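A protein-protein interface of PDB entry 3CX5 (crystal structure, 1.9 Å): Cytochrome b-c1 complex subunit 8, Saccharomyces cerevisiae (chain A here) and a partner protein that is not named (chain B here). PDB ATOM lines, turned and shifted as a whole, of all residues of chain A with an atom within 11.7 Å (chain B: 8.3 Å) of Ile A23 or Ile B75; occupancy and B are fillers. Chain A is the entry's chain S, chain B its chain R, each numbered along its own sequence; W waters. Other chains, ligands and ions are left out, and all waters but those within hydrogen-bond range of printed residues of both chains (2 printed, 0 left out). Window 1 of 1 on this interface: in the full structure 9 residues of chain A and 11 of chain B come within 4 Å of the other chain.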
ATOM      1  N   MET A  15       4.801   1.953   7.768  1.00  0.00           N
ATOM      2  CA  MET A  15       3.483   2.200   7.201  1.00  0.00           C
ATOM      3  C   MET A  15       3.482   2.979   5.877  1.00  0.00           C
ATOM      4  O   MET A  15       2.517   2.912   5.120  1.00  0.00           O
ATOM      5  CB  MET A  15       2.587   2.893   8.236  1.00  0.00           C
ATOM      6  CG  MET A  15       1.096   2.565   8.085  1.00  0.00           C
ATOM      7  SD  MET A  15       0.653   0.819   8.385  1.00  0.00           S
ATOM      8  CE  MET A  15       0.986   0.657  10.140  1.00  0.00           C
ATOM      9  N   GLY A  16       4.551   3.722   5.608  1.00  0.00           N
ATOM     10  CA  GLY A  16       4.634   4.469   4.362  1.00  0.00           C
ATOM     11  C   GLY A  16       4.260   5.933   4.468  1.00  0.00           C
ATOM     12  O   GLY A  16       4.090   6.609   3.443  1.00  0.00           O
ATOM     13  N   GLY A  17       4.102   6.420   5.700  1.00  0.00           N
ATOM     14  CA  GLY A  17       3.771   7.818   5.906  1.00  0.00           C
ATOM     15  C   GLY A  17       5.037   8.640   6.076  1.00  0.00           C
ATOM     16  O   GLY A  17       6.142   8.103   5.976  1.00  0.00           O
ATOM     17  N   PRO A  18       4.917   9.950   6.320  1.00  0.00           N
ATOM     18  CA  PRO A  18       6.109  10.785   6.497  1.00  0.00           C
ATOM     19  C   PRO A  18       6.724  10.558   7.876  1.00  0.00           C
ATOM     20  O   PRO A  18       6.061  10.042   8.778  1.00  0.00           O
ATOM     21  CB  PRO A  18       5.545  12.197   6.371  1.00  0.00           C
ATOM     22  CG  PRO A  18       4.185  12.060   6.972  1.00  0.00           C
ATOM     23  CD  PRO A  18       3.685  10.756   6.400  1.00  0.00           C
ATOM     24  N   LYS A  19       7.998  10.908   8.030  1.00  0.00           N
ATOM     25  CA  LYS A  19       8.665  10.762   9.319  1.00  0.00           C
ATOM     26  C   LYS A  19       7.984  11.702  10.305  1.00  0.00           C
ATOM     27  O   LYS A  19       7.702  12.858   9.982  1.00  0.00           O
ATOM     28  CB  LYS A  19      10.150  11.111   9.210  1.00  0.00           C
ATOM     29  CG  LYS A  19      10.948  10.131   8.377  1.00  0.00           C
ATOM     30  CD  LYS A  19      12.436  10.404   8.464  1.00  0.00           C
ATOM     31  CE  LYS A  19      13.210   9.502   7.505  1.00  0.00           C
ATOM     32  NZ  LYS A  19      12.832   8.068   7.676  1.00  0.00           N
ATOM     33  N   GLN A  20       7.686  11.196  11.492  1.00  0.00           N
ATOM     34  CA  GLN A  20       7.015  11.995  12.509  1.00  0.00           C
ATOM     35  C   GLN A  20       7.986  12.400  13.616  1.00  0.00           C
ATOM     36  O   GLN A  20       8.817  11.594  14.043  1.00  0.00           O
ATOM     37  CB  GLN A  20       5.835  11.213  13.094  1.00  0.00           C
ATOM     38  CG  GLN A  20       4.755  10.825  12.072  1.00  0.00           C
ATOM     39  CD  GLN A  20       3.633  10.004  12.697  1.00  0.00           C
ATOM     40  OE1 GLN A  20       3.392  10.078  13.907  1.00  0.00           O
ATOM     41  NE2 GLN A  20       2.948   9.212  11.876  1.00  0.00           N
ATOM     42  N   LYS A  21       7.872  13.648  14.071  1.00  0.00           N
ATOM     43  CA  LYS A  21       8.735  14.184  15.121  1.00  0.00           C
ATOM     44  C   LYS A  21       8.071  15.422  15.724  1.00  0.00           C
ATOM     45  O   LYS A  21       7.456  16.219  15.003  1.00  0.00           O
ATOM     46  CB  LYS A  21      10.093  14.567  14.515  1.00  0.00           C
ATOM     47  CG  LYS A  21      11.203  14.905  15.499  1.00  0.00           C
ATOM     48  CD  LYS A  21      12.442  15.346  14.725  1.00  0.00           C
ATOM     49  CE  LYS A  21      13.739  15.122  15.489  1.00  0.00           C
ATOM     50  NZ  LYS A  21      13.858  15.974  16.689  1.00  0.00           N
ATOM     51  N   GLY A  22       8.194  15.578  17.042  1.00  0.00           N
ATOM     52  CA  GLY A  22       7.613  16.728  17.719  1.00  0.00           C
ATOM     53  C   GLY A  22       6.203  16.530  18.245  1.00  0.00           C
ATOM     54  O   GLY A  22       5.672  17.377  18.979  1.00  0.00           O
ATOM     55  N   ILE A  23       5.575  15.425  17.854  1.00  0.00           N
ATOM     56  CA  ILE A  23       4.225  15.129  18.310  1.00  0.00           C
ATOM     57  C   ILE A  23       4.307  14.206  19.512  1.00  0.00           C
ATOM     58  O   ILE A  23       5.055  13.231  19.506  1.00  0.00           O
ATOM     59  CB  ILE A  23       3.381  14.416  17.226  1.00  0.00           C
ATOM     60  CG1 ILE A  23       3.360  15.239  15.933  1.00  0.00           C
ATOM     61  CG2 ILE A  23       1.950  14.206  17.723  1.00  0.00           C
ATOM     62  CD1 ILE A  23       2.542  14.600  14.839  1.00  0.00           C
ATOM     63  N   THR A  24       3.567  14.537  20.557  1.00  0.00           N
ATOM     64  CA  THR A  24       3.534  13.689  21.742  1.00  0.00           C
ATOM     65  C   THR A  24       2.069  13.349  22.020  1.00  0.00           C
ATOM     66  O   THR A  24       1.220  14.239  22.037  1.00  0.00           O
ATOM     67  CB  THR A  24       4.135  14.391  22.977  1.00  0.00           C
ATOM     68  OG1 THR A  24       5.503  14.741  22.720  1.00  0.00           O
ATOM     69  CG2 THR A  24       4.084  13.464  24.199  1.00  0.00           C
ATOM     70  N   SER A  25       1.759  12.066  22.171  1.00  0.00           N
ATOM     71  CA  SER A  25       0.388  11.670  22.469  1.00  0.00           C
ATOM     72  C   SER A  25       0.316  11.116  23.880  1.00  0.00           C
ATOM     73  O   SER A  25       1.292  10.592  24.406  1.00  0.00           O
ATOM     74  CB  SER A  25      -0.132  10.624  21.478  1.00  0.00           C
ATOM     75  OG  SER A  25       0.504   9.370  21.649  1.00  0.00           O
ATOM     76  N   TYR A  26      -0.854  11.253  24.484  1.00  0.00           N
ATOM     77  CA  TYR A  26      -1.102  10.772  25.834  1.00  0.00           C
ATOM     78  C   TYR A  26      -2.448  10.066  25.825  1.00  0.00           C
ATOM     79  O   TYR A  26      -3.363  10.465  25.096  1.00  0.00           O
ATOM     80  CB  TYR A  26      -1.185  11.948  26.812  1.00  0.00           C
ATOM     81  CG  TYR A  26       0.014  12.866  26.830  1.00  0.00           C
ATOM     82  CD1 TYR A  26       0.150  13.884  25.891  1.00  0.00           C
ATOM     83  CD2 TYR A  26       0.976  12.764  27.839  1.00  0.00           C
ATOM     84  CE1 TYR A  26       1.210  14.787  25.959  1.00  0.00           C
ATOM     85  CE2 TYR A  26       2.039  13.660  27.916  1.00  0.00           C
ATOM     86  CZ  TYR A  26       2.146  14.668  26.975  1.00  0.00           C
ATOM     87  OH  TYR A  26       3.185  15.558  27.050  1.00  0.00           O
ATOM     88  N   ALA A  27      -2.574   9.026  26.640  1.00  0.00           N
ATOM     89  CA  ALA A  27      -3.816   8.280  26.741  1.00  0.00           C
ATOM     90  C   ALA A  27      -3.921   7.710  28.141  1.00  0.00           C
ATOM     91  O   ALA A  27      -2.921   7.572  28.847  1.00  0.00           O
ATOM     92  CB  ALA A  27      -3.865   7.137  25.699  1.00  0.00           C
ATOM     93  N   LEU B  40     -11.305  21.582  11.305  1.00  0.00           N
ATOM     94  CA  LEU B  40     -10.636  20.350  11.728  1.00  0.00           C
ATOM     95  C   LEU B  40      -9.128  20.596  11.846  1.00  0.00           C
ATOM     96  O   LEU B  40      -8.348  19.666  12.086  1.00  0.00           O
ATOM     97  CB  LEU B  40     -10.915  19.219  10.729  1.00  0.00           C
ATOM     98  CG  LEU B  40     -12.012  18.199  11.075  1.00  0.00           C
ATOM     99  CD1 LEU B  40     -13.110  18.809  11.922  1.00  0.00           C
ATOM    100  CD2 LEU B  40     -12.585  17.605   9.797  1.00  0.00           C
ATOM    101  N   GLY B  41      -8.729  21.859  11.693  1.00  0.00           N
ATOM    102  CA  GLY B  41      -7.325  22.221  11.790  1.00  0.00           C
ATOM    103  C   GLY B  41      -6.525  21.952  10.530  1.00  0.00           C
ATOM    104  O   GLY B  41      -5.296  21.943  10.554  1.00  0.00           O
ATOM    105  N   LEU B  42      -7.215  21.779   9.412  1.00  0.00           N
ATOM    106  CA  LEU B  42      -6.537  21.494   8.155  1.00  0.00           C
ATOM    107  C   LEU B  42      -6.443  22.685   7.208  1.00  0.00           C
ATOM    108  O   LEU B  42      -7.280  23.589   7.246  1.00  0.00           O
ATOM    109  CB  LEU B  42      -7.264  20.358   7.432  1.00  0.00           C
ATOM    110  CG  LEU B  42      -7.228  18.958   8.049  1.00  0.00           C
ATOM    111  CD1 LEU B  42      -8.373  18.124   7.502  1.00  0.00           C
ATOM    112  CD2 LEU B  42      -5.888  18.307   7.758  1.00  0.00           C
ATOM    113  N   SER B  67       6.878  19.589   6.836  1.00  0.00           N
ATOM    114  CA  SER B  67       6.441  18.201   6.755  1.00  0.00           C
ATOM    115  C   SER B  67       5.963  17.728   8.126  1.00  0.00           C
ATOM    116  O   SER B  67       4.928  17.079   8.230  1.00  0.00           O
ATOM    117  CB  SER B  67       7.581  17.306   6.256  1.00  0.00           C
ATOM    118  OG  SER B  67       7.115  15.987   6.040  1.00  0.00           O
ATOM    119  N   TYR B  68       6.710  18.075   9.173  1.00  0.00           N
ATOM    120  CA  TYR B  68       6.333  17.686  10.531  1.00  0.00           C
ATOM    121  C   TYR B  68       5.030  18.368  10.925  1.00  0.00           C
ATOM    122  O   TYR B  68       4.201  17.787  11.639  1.00  0.00           O
ATOM    123  CB  TYR B  68       7.423  18.066  11.539  1.00  0.00           C
ATOM    124  CG  TYR B  68       8.740  17.351  11.369  1.00  0.00           C
ATOM    125  CD1 TYR B  68       9.949  18.030  11.560  1.00  0.00           C
ATOM    126  CD2 TYR B  68       8.789  15.999  11.017  1.00  0.00           C
ATOM    127  CE1 TYR B  68      11.171  17.380  11.406  1.00  0.00           C
ATOM    128  CE2 TYR B  68      10.009  15.341  10.859  1.00  0.00           C
ATOM    129  CZ  TYR B  68      11.190  16.037  11.055  1.00  0.00           C
ATOM    130  OH  TYR B  68      12.386  15.398  10.903  1.00  0.00           O
ATOM    131  N   ALA B  69       4.858  19.605  10.460  1.00  0.00           N
ATOM    132  CA  ALA B  69       3.656  20.371  10.757  1.00  0.00           C
ATOM    133  C   ALA B  69       2.442  19.769  10.053  1.00  0.00           C
ATOM    134  O   ALA B  69       1.357  19.701  10.640  1.00  0.00           O
ATOM    135  CB  ALA B  69       3.841  21.847  10.362  1.00  0.00           C
ATOM    136  N   ARG B  70       2.624  19.338   8.801  1.00  0.00           N
ATOM    137  CA  ARG B  70       1.535  18.723   8.044  1.00  0.00           C
ATOM    138  C   ARG B  70       1.118  17.414   8.725  1.00  0.00           C
ATOM    139  O   ARG B  70      -0.079  17.129   8.858  1.00  0.00           O
ATOM    140  CB  ARG B  70       1.942  18.432   6.589  1.00  0.00           C
ATOM    141  CG  ARG B  70       0.747  18.035   5.705  1.00  0.00           C
ATOM    142  CD  ARG B  70       1.125  17.555   4.298  1.00  0.00           C
ATOM    143  NE  ARG B  70       1.819  16.300   4.420  1.00  0.00           N
ATOM    144  CZ  ARG B  70       1.378  15.121   4.002  1.00  0.00           C
ATOM    145  NH1 ARG B  70       2.133  14.076   4.234  1.00  0.00           N
ATOM    146  NH2 ARG B  70       0.262  14.992   3.289  1.00  0.00           N
ATOM    147  N   ALA B  71       2.106  16.640   9.173  1.00  0.00           N
ATOM    148  CA  ALA B  71       1.847  15.365   9.842  1.00  0.00           C
ATOM    149  C   ALA B  71       0.952  15.586  11.049  1.00  0.00           C
ATOM    150  O   ALA B  71      -0.031  14.862  11.234  1.00  0.00           O
ATOM    151  CB  ALA B  71       3.145  14.694  10.266  1.00  0.00           C
ATOM    152  N   TYR B  72       1.275  16.603  11.846  1.00  0.00           N
ATOM    153  CA  TYR B  72       0.478  16.919  13.034  1.00  0.00           C
ATOM    154  C   TYR B  72      -0.968  17.300  12.706  1.00  0.00           C
ATOM    155  O   TYR B  72      -1.899  16.832  13.370  1.00  0.00           O
ATOM    156  CB  TYR B  72       1.120  18.035  13.864  1.00  0.00           C
ATOM    157  CG  TYR B  72       0.261  18.460  15.044  1.00  0.00           C
ATOM    158  CD1 TYR B  72      -0.012  17.575  16.086  1.00  0.00           C
ATOM    159  CD2 TYR B  72      -0.291  19.741  15.106  1.00  0.00           C
ATOM    160  CE1 TYR B  72      -0.814  17.956  17.166  1.00  0.00           C
ATOM    161  CE2 TYR B  72      -1.098  20.133  16.183  1.00  0.00           C
ATOM    162  CZ  TYR B  72      -1.350  19.237  17.203  1.00  0.00           C
ATOM    163  OH  TYR B  72      -2.132  19.621  18.266  1.00  0.00           O
ATOM    164  N   ARG B  73      -1.156  18.146  11.694  1.00  0.00           N
ATOM    165  CA  ARG B  73      -2.499  18.572  11.306  1.00  0.00           C
ATOM    166  C   ARG B  73      -3.344  17.378  10.850  1.00  0.00           C
ATOM    167  O   ARG B  73      -4.515  17.272  11.200  1.00  0.00           O
ATOM    168  CB  ARG B  73      -2.451  19.651  10.202  1.00  0.00           C
ATOM    169  CG  ARG B  73      -1.829  20.994  10.658  1.00  0.00           C
ATOM    170  CD  ARG B  73      -2.075  22.135   9.661  1.00  0.00           C
ATOM    171  NE  ARG B  73      -1.523  21.869   8.333  1.00  0.00           N
ATOM    172  CZ  ARG B  73      -0.267  22.117   7.967  1.00  0.00           C
ATOM    173  NH1 ARG B  73       0.126  21.831   6.734  1.00  0.00           N
ATOM    174  NH2 ARG B  73       0.597  22.662   8.820  1.00  0.00           N
ATOM    175  N   ILE B  74      -2.737  16.469  10.094  1.00  0.00           N
ATOM    176  CA  ILE B  74      -3.443  15.290   9.606  1.00  0.00           C
ATOM    177  C   ILE B  74      -3.841  14.379  10.773  1.00  0.00           C
ATOM    178  O   ILE B  74      -5.005  13.985  10.895  1.00  0.00           O
ATOM    179  CB  ILE B  74      -2.579  14.539   8.550  1.00  0.00           C
ATOM    180  CG1 ILE B  74      -2.536  15.377   7.262  1.00  0.00           C
ATOM    181  CG2 ILE B  74      -3.128  13.122   8.306  1.00  0.00           C
ATOM    182  CD1 ILE B  74      -1.578  14.872   6.191  1.00  0.00           C
ATOM    183  N   ILE B  75      -2.902  14.134  11.682  1.00  0.00           N
ATOM    184  CA  ILE B  75      -3.168  13.277  12.838  1.00  0.00           C
ATOM    185  C   ILE B  75      -4.237  13.874  13.742  1.00  0.00           C
ATOM    186  O   ILE B  75      -5.163  13.180  14.166  1.00  0.00           O
ATOM    187  CB  ILE B  75      -1.878  12.997  13.629  1.00  0.00           C
ATOM    188  CG1 ILE B  75      -0.979  12.058  12.810  1.00  0.00           C
ATOM    189  CG2 ILE B  75      -2.197  12.345  14.975  1.00  0.00           C
ATOM    190  CD1 ILE B  75       0.455  12.029  13.260  1.00  0.00           C
ATOM    191  N   ARG B  76      -4.094  15.158  14.056  1.00  0.00           N
ATOM    192  CA  ARG B  76      -5.063  15.853  14.897  1.00  0.00           C
ATOM    193  C   ARG B  76      -6.453  15.844  14.241  1.00  0.00           C
ATOM    194  O   ARG B  76      -7.465  15.675  14.919  1.00  0.00           O
ATOM    195  CB  ARG B  76      -4.579  17.281  15.167  1.00  0.00           C
ATOM    196  CG  ARG B  76      -5.631  18.236  15.679  1.00  0.00           C
ATOM    197  CD  ARG B  76      -5.528  19.558  14.912  1.00  0.00           C
ATOM    198  NE  ARG B  76      -4.716  20.546  15.588  1.00  0.00           N
ATOM    199  CZ  ARG B  76      -4.243  21.666  15.040  1.00  0.00           C
ATOM    200  NH1 ARG B  76      -3.525  22.488  15.789  1.00  0.00           N
ATOM    201  NH2 ARG B  76      -4.428  21.954  13.756  1.00  0.00           N
ATOM    202  N   ALA B  77      -6.495  15.997  12.917  1.00  0.00           N
ATOM    203  CA  ALA B  77      -7.758  15.978  12.188  1.00  0.00           C
ATOM    204  C   ALA B  77      -8.428  14.603  12.297  1.00  0.00           C
ATOM    205  O   ALA B  77      -9.645  14.521  12.448  1.00  0.00           O
ATOM    206  CB  ALA B  77      -7.537  16.365  10.710  1.00  0.00           C
ATOM    207  N   HIS B  78      -7.638  13.528  12.233  1.00  0.00           N
ATOM    208  CA  HIS B  78      -8.192  12.182  12.358  1.00  0.00           C
ATOM    209  C   HIS B  78      -8.756  11.951  13.754  1.00  0.00           C
ATOM    210  O   HIS B  78      -9.829  11.382  13.901  1.00  0.00           O
ATOM    211  CB  HIS B  78      -7.145  11.105  12.025  1.00  0.00           C
ATOM    212  CG  HIS B  78      -6.997  10.847  10.557  1.00  0.00           C
ATOM    213  ND1 HIS B  78      -5.806  11.013   9.886  1.00  0.00           N
ATOM    214  CD2 HIS B  78      -7.899  10.451   9.629  1.00  0.00           C
ATOM    215  CE1 HIS B  78      -5.979  10.734   8.606  1.00  0.00           C
ATOM    216  NE2 HIS B  78      -7.242  10.390   8.424  1.00  0.00           N
ATOM    217  N   GLN B  79      -8.041  12.422  14.771  1.00  0.00           N
ATOM    218  CA  GLN B  79      -8.485  12.262  16.155  1.00  0.00           C
ATOM    219  C   GLN B  79      -9.782  13.039  16.416  1.00  0.00           C
ATOM    220  O   GLN B  79     -10.698  12.527  17.050  1.00  0.00           O
ATOM    221  CB  GLN B  79      -7.396  12.731  17.127  1.00  0.00           C
ATOM    222  CG  GLN B  79      -7.803  12.657  18.595  1.00  0.00           C
ATOM    223  CD  GLN B  79      -8.079  11.234  19.058  1.00  0.00           C
ATOM    224  OE1 GLN B  79      -7.434  10.279  18.604  1.00  0.00           O
ATOM    225  NE2 GLN B  79      -9.033  11.084  19.980  1.00  0.00           N
ATOM    226  N   THR B  80      -9.853  14.261  15.898  1.00  0.00           N
ATOM    227  CA  THR B  80     -11.026  15.121  16.070  1.00  0.00           C
ATOM    228  C   THR B  80     -12.224  14.515  15.350  1.00  0.00           C
ATOM    229  O   THR B  80     -13.336  14.482  15.880  1.00  0.00           O
ATOM    230  CB  THR B  80     -10.755  16.538  15.508  1.00  0.00           C
ATOM    231  OG1 THR B  80      -9.509  17.026  16.032  1.00  0.00           O
ATOM    232  CG2 THR B  80     -11.861  17.494  15.914  1.00  0.00           C
ATOM    233  N   GLU B  81     -11.969  13.996  14.155  1.00  0.00           N
ATOM    234  CA  GLU B  81     -13.001  13.368  13.341  1.00  0.00           C
ATOM    235  C   GLU B  81     -13.601  12.132  14.031  1.00  0.00           C
ATOM    236  O   GLU B  81     -14.829  11.987  14.116  1.00  0.00           O
ATOM    237  CB  GLU B  81     -12.407  12.983  11.981  1.00  0.00           C
ATOM    238  CG  GLU B  81     -13.358  12.285  11.029  1.00  0.00           C
ATOM    239  CD  GLU B  81     -14.560  13.135  10.652  1.00  0.00           C
ATOM    240  OE1 GLU B  81     -15.647  12.553  10.480  1.00  0.00           O
ATOM    241  OE2 GLU B  81     -14.430  14.375  10.518  1.00  0.00           O
ATOM    242  N   LEU B  82     -12.742  11.271  14.567  1.00  0.00           N
ATOM    243  CA  LEU B  82     -13.226  10.060  15.217  1.00  0.00           C
ATOM    244  C   LEU B  82     -14.038  10.326  16.492  1.00  0.00           C
ATOM    245  O   LEU B  82     -14.835   9.479  16.905  1.00  0.00           O
ATOM    246  CB  LEU B  82     -12.080   9.058  15.454  1.00  0.00           C
ATOM    247  CG  LEU B  82     -11.007   9.280  16.521  1.00  0.00           C
ATOM    248  CD1 LEU B  82     -11.560   8.909  17.890  1.00  0.00           C
ATOM    249  CD2 LEU B  82      -9.776   8.415  16.215  1.00  0.00           C
HETATM  250  O   HOH W   1       5.477  15.348  12.901  1.00  0.00           O
HETATM  251  O   HOH W   2       8.058  14.483   7.863  1.00  0.00           O
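Water W2 bridges OG of Ser B67 (2.5 Å) and O of Lys A19 (2.7 Å).
Water W1 lies within hydrogen-bond range of O of Lys A21 (3.0 Å) and O of Tyr B68 (3.0 Å).
Printed residues of chain B within 4 Å of Lys A21: Tyr B68.
No residue of chain B comes within 4 Å of Gly A22.
Printed residues of chain A within 4 Å of Tyr B68: Lys A19 (3.5 Å) and Lys A21 (3.7 Å).
Of the printed residues of chain A, Arg B70 touches Pro A18.
Tyr B72 touches just one residue of chain A: Ile A23.
Ile B74 touches none of the printed residues of chain A.
No residue of chain A comes within 4 Å of Ala B77.
His B78 touches none of the printed residues of chain A.
No residue of chain A comes within 4 Å of Gln B79.
The nearest residue of chain B that does not touch Ile A23 is Ala B71 (4.2 Å).
The nearest printed residue of chain B that does not touch Gln A20 is Tyr B68 (4.5 Å).
Arg B70 touches Pro A18 (NH1 to CG, 3.97 Å).
CD2 of Tyr B68 touches O of Lys A19, 3.5 Å away.
OE1 of Gln A20 touches CD1 of Ile B75, 3.6 Å away.
CE2 of Tyr B68 touches CB of Lys A21, at 3.7 Å.
Ile A23 touches Tyr B72.
CD1 of Ile A23 touches CD1 of Ile B75, at 3.7 Å.
Of the 19 printed residues of chain B, 4 touch a printed residue of chain A.
Printed residues of chain B that touch a printed residue of chain A: Tyr B68, Arg B70, Tyr B72 and Ile B75.
Of the 13 printed residues of chain A, 5 touch a printed residue of chain B.
Printed residues of chain A that touch a printed residue of chain B: Pro A18, Lys A19, Gln A20, Lys A21 and Ile A23.
Hydrophobic or aromatic side chains of chain A that line the printed part of chain B: Pro A18 and Ile A23.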
